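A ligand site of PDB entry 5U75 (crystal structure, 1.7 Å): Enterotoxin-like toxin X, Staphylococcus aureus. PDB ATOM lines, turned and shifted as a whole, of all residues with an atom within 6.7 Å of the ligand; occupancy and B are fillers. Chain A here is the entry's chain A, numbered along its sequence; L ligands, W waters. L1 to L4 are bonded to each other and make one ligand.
An oxygen (O1) of LIG L1 lies within hydrogen-bond range of the side-chain hydroxyl (OG1) of Thr 130.
The side-chain amide nitrogen (NE2) of Gln 138 is in hydrogen-bond range of an oxygen (O5) of LG2 L2 (3.0 Å).
The backbone NH (N) of Thr 130 lies within hydrogen-bond range of an oxygen (O2) of LIG L1, at 2.8 Å.
OE2 of Glu 132 lies within hydrogen-bond range of O5 of LG2 L2.
The guanidinium group of Arg 141 lies within salt-bridge range of an oxygen (O2) of LIG L1, at 3.5 Å.
N1 of LIG L1 lies within hydrogen-bond range of O of Lys 128, 2.9 Å away.
An oxygen (O1) of LG4 L4 is in hydrogen-bond range of the side-chain amino group of Lys 135, at 2.9 Å.
O4 of LG3 L3 sits at hydrogen-bond distance from OD1 of Asn 140, at 2.8 Å.
N of Leu 92 lies within hydrogen-bond range of O of Val 144 (2.8 Å).
NH1 of Arg 141 is in hydrogen-bond range of OE1 of Gln 138 (3.1 Å).
O of Thr 130 lies within hydrogen-bond range of NH2 of Arg 141.
The side-chain carboxylate (OE2) of Glu 132 is in salt-bridge range of the side-chain amino group (NZ) of Lys 135.
CD2 of Leu 92 touches O7 of LIG L1 (3.6 Å).
Tyr 129 touches the ligand.
Val 144 touches the ligand.
Hydrophobic or aromatic side chains that line the ligand: Leu 92, Tyr 129 and Val 144.
Of the 18 residues printed, 10 come within 4 Å of the ligand.
The nearest printed residue that does not touch the ligand is Gly 127 (5.1 Å).
Water W3 lies within hydrogen-bond range of O5 of LG2 L2, N of Glu 132, NH1 of Arg 141, OE1 of Gln 138 and O of Thr 130.
Water W6 lies within hydrogen-bond range of an oxygen (O3) of LIG L1 and the backbone NH (N) of Lys 128.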
ATOM      1  N   LEU A  92      15.610  35.497 -30.541  1.00  0.00           N
ATOM      2  CA  LEU A  92      15.263  34.253 -29.850  1.00  0.00           C
ATOM      3  C   LEU A  92      14.036  34.433 -28.943  1.00  0.00           C
ATOM      4  O   LEU A  92      13.222  33.518 -28.813  1.00  0.00           O
ATOM      5  CB  LEU A  92      16.468  33.708 -29.083  1.00  0.00           C
ATOM      6  CG  LEU A  92      16.269  32.367 -28.346  1.00  0.00           C
ATOM      7  CD1 LEU A  92      15.714  31.302 -29.283  1.00  0.00           C
ATOM      8  CD2 LEU A  92      17.609  31.950 -27.762  1.00  0.00           C
ATOM      9  N   ASN A 118      13.057  19.187 -23.381  1.00  0.00           N
ATOM     10  CA  ASN A 118      13.505  20.292 -24.204  1.00  0.00           C
ATOM     11  C   ASN A 118      12.818  20.351 -25.542  1.00  0.00           C
ATOM     12  O   ASN A 118      12.547  19.321 -26.171  1.00  0.00           O
ATOM     13  CB  ASN A 118      14.980  20.205 -24.467  1.00  0.00           C
ATOM     14  CG  ASN A 118      15.793  20.288 -23.195  1.00  0.00           C
ATOM     15  OD1 ASN A 118      15.376  20.911 -22.213  1.00  0.00           O
ATOM     16  ND2 ASN A 118      16.951  19.635 -23.193  1.00  0.00           N
ATOM     17  N   VAL A 120      13.923  21.880 -29.148  1.00  0.00           N
ATOM     18  CA  VAL A 120      15.186  22.234 -29.769  1.00  0.00           C
ATOM     19  C   VAL A 120      14.987  22.819 -31.163  1.00  0.00           C
ATOM     20  O   VAL A 120      14.441  22.163 -32.033  1.00  0.00           O
ATOM     21  CB  VAL A 120      16.155  21.031 -29.829  1.00  0.00           C
ATOM     22  CG1 VAL A 120      17.495  21.444 -30.427  1.00  0.00           C
ATOM     23  CG2 VAL A 120      16.326  20.434 -28.431  1.00  0.00           C
ATOM     24  N   THR A 123      19.320  24.082 -36.627  1.00  0.00           N
ATOM     25  CA  THR A 123      19.689  24.918 -37.775  1.00  0.00           C
ATOM     26  C   THR A 123      20.217  24.065 -38.912  1.00  0.00           C
ATOM     27  O   THR A 123      20.592  22.889 -38.728  1.00  0.00           O
ATOM     28  CB  THR A 123      20.689  26.048 -37.445  1.00  0.00           C
ATOM     29  OG1 THR A 123      22.027  25.549 -37.372  1.00  0.00           O
ATOM     30  CG2 THR A 123      20.330  26.755 -36.147  1.00  0.00           C
ATOM     31  N   GLY A 127      23.530  23.585 -35.983  1.00  0.00           N
ATOM     32  CA  GLY A 127      23.420  24.353 -34.758  1.00  0.00           C
ATOM     33  C   GLY A 127      22.140  24.028 -33.996  1.00  0.00           C
ATOM     34  O   GLY A 127      21.185  23.454 -34.541  1.00  0.00           O
ATOM     35  N   LYS A 128      22.133  24.353 -32.712  1.00  0.00           N
ATOM     36  CA  LYS A 128      20.906  24.274 -31.955  1.00  0.00           C
ATOM     37  C   LYS A 128      20.695  25.418 -30.960  1.00  0.00           C
ATOM     38  O   LYS A 128      21.656  26.036 -30.509  1.00  0.00           O
ATOM     39  CB  LYS A 128      20.818  22.938 -31.229  1.00  0.00           C
ATOM     40  CG  LYS A 128      21.866  22.757 -30.143  1.00  0.00           C
ATOM     41  CD  LYS A 128      21.824  21.326 -29.628  1.00  0.00           C
ATOM     42  CE  LYS A 128      22.801  21.124 -28.492  1.00  0.00           C
ATOM     43  NZ  LYS A 128      22.531  19.844 -27.768  1.00  0.00           N
ATOM     44  N   TYR A 129      19.425  25.666 -30.659  1.00  0.00           N
ATOM     45  CA  TYR A 129      18.994  26.517 -29.565  1.00  0.00           C
ATOM     46  C   TYR A 129      18.004  25.689 -28.759  1.00  0.00           C
ATOM     47  O   TYR A 129      16.959  25.281 -29.269  1.00  0.00           O
ATOM     48  CB  TYR A 129      18.328  27.812 -30.060  1.00  0.00           C
ATOM     49  CG  TYR A 129      19.155  28.609 -31.030  1.00  0.00           C
ATOM     50  CD1 TYR A 129      20.081  29.557 -30.576  1.00  0.00           C
ATOM     51  CD2 TYR A 129      19.027  28.429 -32.411  1.00  0.00           C
ATOM     52  CE1 TYR A 129      20.853  30.305 -31.456  1.00  0.00           C
ATOM     53  CE2 TYR A 129      19.771  29.183 -33.311  1.00  0.00           C
ATOM     54  CZ  TYR A 129      20.697  30.112 -32.834  1.00  0.00           C
ATOM     55  OH  TYR A 129      21.441  30.836 -33.733  1.00  0.00           O
ATOM     56  N   THR A 130      18.324  25.482 -27.483  1.00  0.00           N
ATOM     57  CA  THR A 130      17.564  24.601 -26.611  1.00  0.00           C
ATOM     58  C   THR A 130      16.669  25.381 -25.681  1.00  0.00           C
ATOM     59  O   THR A 130      17.125  26.279 -24.959  1.00  0.00           O
ATOM     60  CB  THR A 130      18.497  23.668 -25.782  1.00  0.00           C
ATOM     61  OG1 THR A 130      19.382  22.971 -26.643  1.00  0.00           O
ATOM     62  CG2 THR A 130      17.676  22.703 -24.953  1.00  0.00           C
ATOM     63  N   LEU A 131      15.388  25.044 -25.696  1.00  0.00           N
ATOM     64  CA  LEU A 131      14.365  25.665 -24.910  1.00  0.00           C
ATOM     65  C   LEU A 131      13.855  24.669 -23.878  1.00  0.00           C
ATOM     66  O   LEU A 131      13.065  23.764 -24.195  1.00  0.00           O
ATOM     67  CB  LEU A 131      13.216  26.124 -25.801  1.00  0.00           C
ATOM     68  CG  LEU A 131      13.607  26.872 -27.074  1.00  0.00           C
ATOM     69  CD1 LEU A 131      12.326  27.172 -27.835  1.00  0.00           C
ATOM     70  CD2 LEU A 131      14.370  28.154 -26.782  1.00  0.00           C
ATOM     71  N   GLU A 132      14.261  24.867 -22.632  1.00  0.00           N
ATOM     72  CA  GLU A 132      13.809  24.013 -21.536  1.00  0.00           C
ATOM     73  C   GLU A 132      12.368  24.339 -21.165  1.00  0.00           C
ATOM     74  O   GLU A 132      12.059  25.466 -20.768  1.00  0.00           O
ATOM     75  CB  GLU A 132      14.737  24.188 -20.333  1.00  0.00           C
ATOM     76  CG  GLU A 132      16.176  23.855 -20.605  1.00  0.00           C
ATOM     77  CD  GLU A 132      17.005  23.841 -19.336  1.00  0.00           C
ATOM     78  OE1 GLU A 132      16.814  22.898 -18.554  1.00  0.00           O
ATOM     79  OE2 GLU A 132      17.823  24.772 -19.129  1.00  0.00           O
ATOM     80  N   HIS A 134      10.191  23.573 -18.799  1.00  0.00           N
ATOM     81  CA  HIS A 134       9.682  23.690 -17.441  1.00  0.00           C
ATOM     82  C   HIS A 134       9.778  25.115 -16.858  1.00  0.00           C
ATOM     83  O   HIS A 134       9.267  25.372 -15.760  1.00  0.00           O
ATOM     84  CB  HIS A 134      10.417  22.690 -16.521  1.00  0.00           C
ATOM     85  CG  HIS A 134      11.849  23.010 -16.289  1.00  0.00           C
ATOM     86  ND1 HIS A 134      12.850  22.683 -17.183  1.00  0.00           N
ATOM     87  CD2 HIS A 134      12.459  23.647 -15.254  1.00  0.00           C
ATOM     88  CE1 HIS A 134      14.010  23.085 -16.694  1.00  0.00           C
ATOM     89  NE2 HIS A 134      13.792  23.681 -15.543  1.00  0.00           N
ATOM     90  N   LYS A 135      10.432  26.026 -17.585  1.00  0.00           N
ATOM     91  CA  LYS A 135      10.639  27.379 -17.117  1.00  0.00           C
ATOM     92  C   LYS A 135      10.673  28.331 -18.316  1.00  0.00           C
ATOM     93  O   LYS A 135      10.796  27.913 -19.459  1.00  0.00           O
ATOM     94  CB  LYS A 135      11.963  27.470 -16.332  1.00  0.00           C
ATOM     95  CG  LYS A 135      13.200  27.094 -17.115  1.00  0.00           C
ATOM     96  CD  LYS A 135      14.475  27.134 -16.280  1.00  0.00           C
ATOM     97  CE  LYS A 135      15.683  26.816 -17.146  1.00  0.00           C
ATOM     98  NZ  LYS A 135      16.962  26.677 -16.381  1.00  0.00           N
ATOM     99  N   LEU A 137      12.117  31.237 -20.929  1.00  0.00           N
ATOM    100  CA  LEU A 137      13.415  31.544 -21.524  1.00  0.00           C
ATOM    101  C   LEU A 137      14.188  32.473 -20.589  1.00  0.00           C
ATOM    102  O   LEU A 137      13.621  33.450 -20.076  1.00  0.00           O
ATOM    103  CB  LEU A 137      13.212  32.261 -22.861  1.00  0.00           C
ATOM    104  CG  LEU A 137      14.436  32.624 -23.694  1.00  0.00           C
ATOM    105  CD1 LEU A 137      15.109  31.390 -24.254  1.00  0.00           C
ATOM    106  CD2 LEU A 137      14.011  33.565 -24.826  1.00  0.00           C
ATOM    107  N   GLN A 138      15.475  32.218 -20.429  1.00  0.00           N
ATOM    108  CA  GLN A 138      16.336  33.067 -19.600  1.00  0.00           C
ATOM    109  C   GLN A 138      16.458  34.456 -20.257  1.00  0.00           C
ATOM    110  O   GLN A 138      16.617  34.565 -21.483  1.00  0.00           O
ATOM    111  CB  GLN A 138      17.712  32.445 -19.408  1.00  0.00           C
ATOM    112  CG  GLN A 138      17.692  31.102 -18.678  1.00  0.00           C
ATOM    113  CD  GLN A 138      17.819  29.898 -19.616  1.00  0.00           C
ATOM    114  OE1 GLN A 138      17.110  29.806 -20.624  1.00  0.00           O
ATOM    115  NE2 GLN A 138      18.712  28.974 -19.287  1.00  0.00           N
ATOM    116  N   ASN A 140      18.775  36.692 -20.366  1.00  0.00           N
ATOM    117  CA  ASN A 140      20.019  36.958 -21.097  1.00  0.00           C
ATOM    118  C   ASN A 140      20.084  36.377 -22.531  1.00  0.00           C
ATOM    119  O   ASN A 140      21.023  36.664 -23.277  1.00  0.00           O
ATOM    120  CB  ASN A 140      21.274  36.589 -20.264  1.00  0.00           C
ATOM    121  CG  ASN A 140      21.502  35.076 -20.135  1.00  0.00           C
ATOM    122  OD1 ASN A 140      20.893  34.268 -20.817  1.00  0.00           O
ATOM    123  ND2 ASN A 140      22.450  34.699 -19.262  1.00  0.00           N
ATOM    124  N   ARG A 141      19.096  35.563 -22.898  1.00  0.00           N
ATOM    125  CA  ARG A 141      19.003  34.961 -24.241  1.00  0.00           C
ATOM    126  C   ARG A 141      18.040  35.690 -25.173  1.00  0.00           C
ATOM    127  O   ARG A 141      17.984  35.367 -26.350  1.00  0.00           O
ATOM    128  CB  ARG A 141      18.525  33.510 -24.121  1.00  0.00           C
ATOM    129  CG  ARG A 141      19.366  32.684 -23.163  1.00  0.00           C
ATOM    130  CD  ARG A 141      18.832  31.276 -22.994  1.00  0.00           C
ATOM    131  NE  ARG A 141      18.878  30.519 -24.248  1.00  0.00           N
ATOM    132  CZ  ARG A 141      18.249  29.349 -24.451  1.00  0.00           C
ATOM    133  NH1 ARG A 141      17.519  28.804 -23.495  1.00  0.00           N
ATOM    134  NH2 ARG A 141      18.346  28.766 -25.639  1.00  0.00           N
ATOM    135  N   GLU A 142      17.295  36.670 -24.653  1.00  0.00           N
ATOM    136  CA  GLU A 142      16.202  37.290 -25.412  1.00  0.00           C
ATOM    137  C   GLU A 142      16.626  37.941 -26.702  1.00  0.00           C
ATOM    138  O   GLU A 142      15.858  37.932 -27.653  1.00  0.00           O
ATOM    139  CB  GLU A 142      15.474  38.302 -24.567  1.00  0.00           C
ATOM    140  CG  GLU A 142      14.644  37.647 -23.479  1.00  0.00           C
ATOM    141  CD  GLU A 142      13.953  38.634 -22.565  1.00  0.00           C
ATOM    142  OE1 GLU A 142      14.062  39.855 -22.788  1.00  0.00           O
ATOM    143  OE2 GLU A 142      13.300  38.181 -21.626  1.00  0.00           O
ATOM    144  N   VAL A 144      19.325  37.300 -28.781  1.00  0.00           N
ATOM    145  CA  VAL A 144      20.126  36.514 -29.713  1.00  0.00           C
ATOM    146  C   VAL A 144      19.424  36.553 -31.068  1.00  0.00           C
ATOM    147  O   VAL A 144      18.220  36.364 -31.132  1.00  0.00           O
ATOM    148  CB  VAL A 144      20.279  35.049 -29.217  1.00  0.00           C
ATOM    149  CG1 VAL A 144      20.911  34.140 -30.286  1.00  0.00           C
ATOM    150  CG2 VAL A 144      21.112  35.012 -27.941  1.00  0.00           C
HETATM  151  C1  LIG L   1      21.792  25.641 -26.446  1.00  0.00           C
HETATM  152  C2  LIG L   1      23.165  26.206 -26.087  1.00  0.00           C
HETATM  153  C3  LIG L   1      24.314  25.476 -26.811  1.00  0.00           C
HETATM  154  C4  LIG L   1      24.305  25.775 -28.306  1.00  0.00           C
HETATM  155  C5  LIG L   1      24.258  27.278 -28.616  1.00  0.00           C
HETATM  156  C6  LIG L   1      23.119  27.917 -27.824  1.00  0.00           C
HETATM  157  C7  LIG L   1      22.973  29.441 -27.894  1.00  0.00           C
HETATM  158  C8  LIG L   1      21.906  29.925 -26.920  1.00  0.00           C
HETATM  159  C9  LIG L   1      21.486  31.360 -27.239  1.00  0.00           C
HETATM  160  C10 LIG L   1      24.596  28.545 -30.679  1.00  0.00           C
HETATM  161  C11 LIG L   1      24.312  28.641 -32.140  1.00  0.00           C
HETATM  162  N1  LIG L   1      24.066  27.485 -30.039  1.00  0.00           N
HETATM  163  O1  LIG L   1      21.686  24.417 -26.654  1.00  0.00           O
HETATM  164  O2  LIG L   1      20.800  26.427 -26.484  1.00  0.00           O
HETATM  165  O3  LIG L   1      25.436  25.234 -28.977  1.00  0.00           O
HETATM  166  O4  LIG L   1      23.236  27.616 -26.438  1.00  0.00           O
HETATM  167  O5  LIG L   1      24.240  30.083 -27.664  1.00  0.00           O
HETATM  168  O6  LIG L   1      20.727  29.117 -27.004  1.00  0.00           O
HETATM  169  O7  LIG L   1      20.796  31.881 -26.114  1.00  0.00           O
HETATM  170  O8  LIG L   1      25.261  29.415 -30.102  1.00  0.00           O
HETATM  171  C1  LG2 L   2      22.206  28.185 -21.741  1.00  0.00           C
HETATM  172  C2  LG2 L   2      23.150  27.460 -22.691  1.00  0.00           C
HETATM  173  C3  LG2 L   2      22.383  26.827 -23.849  1.00  0.00           C
HETATM  174  C4  LG2 L   2      21.271  25.936 -23.276  1.00  0.00           C
HETATM  175  C5  LG2 L   2      20.373  26.714 -22.322  1.00  0.00           C
HETATM  176  C6  LG2 L   2      19.297  25.802 -21.753  1.00  0.00           C
HETATM  177  O1  LG2 L   2      24.152  28.349 -23.186  1.00  0.00           O
HETATM  178  O2  LG2 L   2      23.300  26.087 -24.668  1.00  0.00           O
HETATM  179  O3  LG2 L   2      21.882  24.827 -22.638  1.00  0.00           O
HETATM  180  O4  LG2 L   2      21.145  27.319 -21.278  1.00  0.00           O
HETATM  181  O5  LG2 L   2      18.408  26.497 -20.869  1.00  0.00           O
HETATM  182  C1  LG3 L   3      22.725  31.528 -17.676  1.00  0.00           C
HETATM  183  C2  LG3 L   3      21.844  30.308 -17.511  1.00  0.00           C
HETATM  184  C3  LG3 L   3      22.406  29.146 -18.334  1.00  0.00           C
HETATM  185  C4  LG3 L   3      22.413  29.602 -19.802  1.00  0.00           C
HETATM  186  C5  LG3 L   3      23.237  30.890 -19.948  1.00  0.00           C
HETATM  187  C6  LG3 L   3      23.150  31.455 -21.361  1.00  0.00           C
HETATM  188  C7  LG3 L   3      20.503  29.773 -15.518  1.00  0.00           C
HETATM  189  C8  LG3 L   3      20.555  29.410 -14.053  1.00  0.00           C
HETATM  190  O1  LG3 L   3      22.738  31.897 -19.061  1.00  0.00           O
HETATM  191  O2  LG3 L   3      21.594  27.973 -18.159  1.00  0.00           O
HETATM  192  O3  LG3 L   3      22.990  28.599 -20.636  1.00  0.00           O
HETATM  193  O4  LG3 L   3      21.772  31.776 -21.596  1.00  0.00           O
HETATM  194  O5  LG3 L   3      19.436  29.883 -16.104  1.00  0.00           O
HETATM  195  N1  LG3 L   3      21.697  29.959 -16.108  1.00  0.00           N
HETATM  196  O6  LG3 L   3      24.068  31.237 -17.287  1.00  0.00           O
HETATM  197  C1  LG4 L   4      22.131  26.984 -17.263  1.00  0.00           C
HETATM  198  C2  LG4 L   4      21.102  25.879 -17.038  1.00  0.00           C
HETATM  199  C3  LG4 L   4      20.923  25.035 -18.282  1.00  0.00           C
HETATM  200  C4  LG4 L   4      22.259  24.473 -18.741  1.00  0.00           C
HETATM  201  C5  LG4 L   4      23.217  25.638 -18.979  1.00  0.00           C
HETATM  202  C6  LG4 L   4      24.590  25.186 -19.426  1.00  0.00           C
HETATM  203  O1  LG4 L   4      19.833  26.436 -16.702  1.00  0.00           O
HETATM  204  O2  LG4 L   4      19.977  23.990 -18.022  1.00  0.00           O
HETATM  205  O3  LG4 L   4      22.757  23.593 -17.729  1.00  0.00           O
HETATM  206  O4  LG4 L   4      23.343  26.444 -17.805  1.00  0.00           O
HETATM  207  O   HOH W   1      22.970  22.444 -25.228  1.00  0.00           O
HETATM  208  O   HOH W   2      25.972  28.694 -21.031  1.00  0.00           O
HETATM  209  O   HOH W   3      15.912  27.066 -21.923  1.00  0.00           O
HETATM  210  O   HOH W   4      24.348  23.623 -22.995  1.00  0.00           O
HETATM  211  O   HOH W   5      22.760  32.646 -24.472  1.00  0.00           O
HETATM  212  O   HOH W   6      24.760  24.770 -31.647  1.00  0.00           O
HETATM  213  O   HOH W   7      20.471  22.416 -22.410  1.00  0.00           O
HETATM  214  O   HOH W   8      25.408  32.028 -30.808  1.00  0.00           O
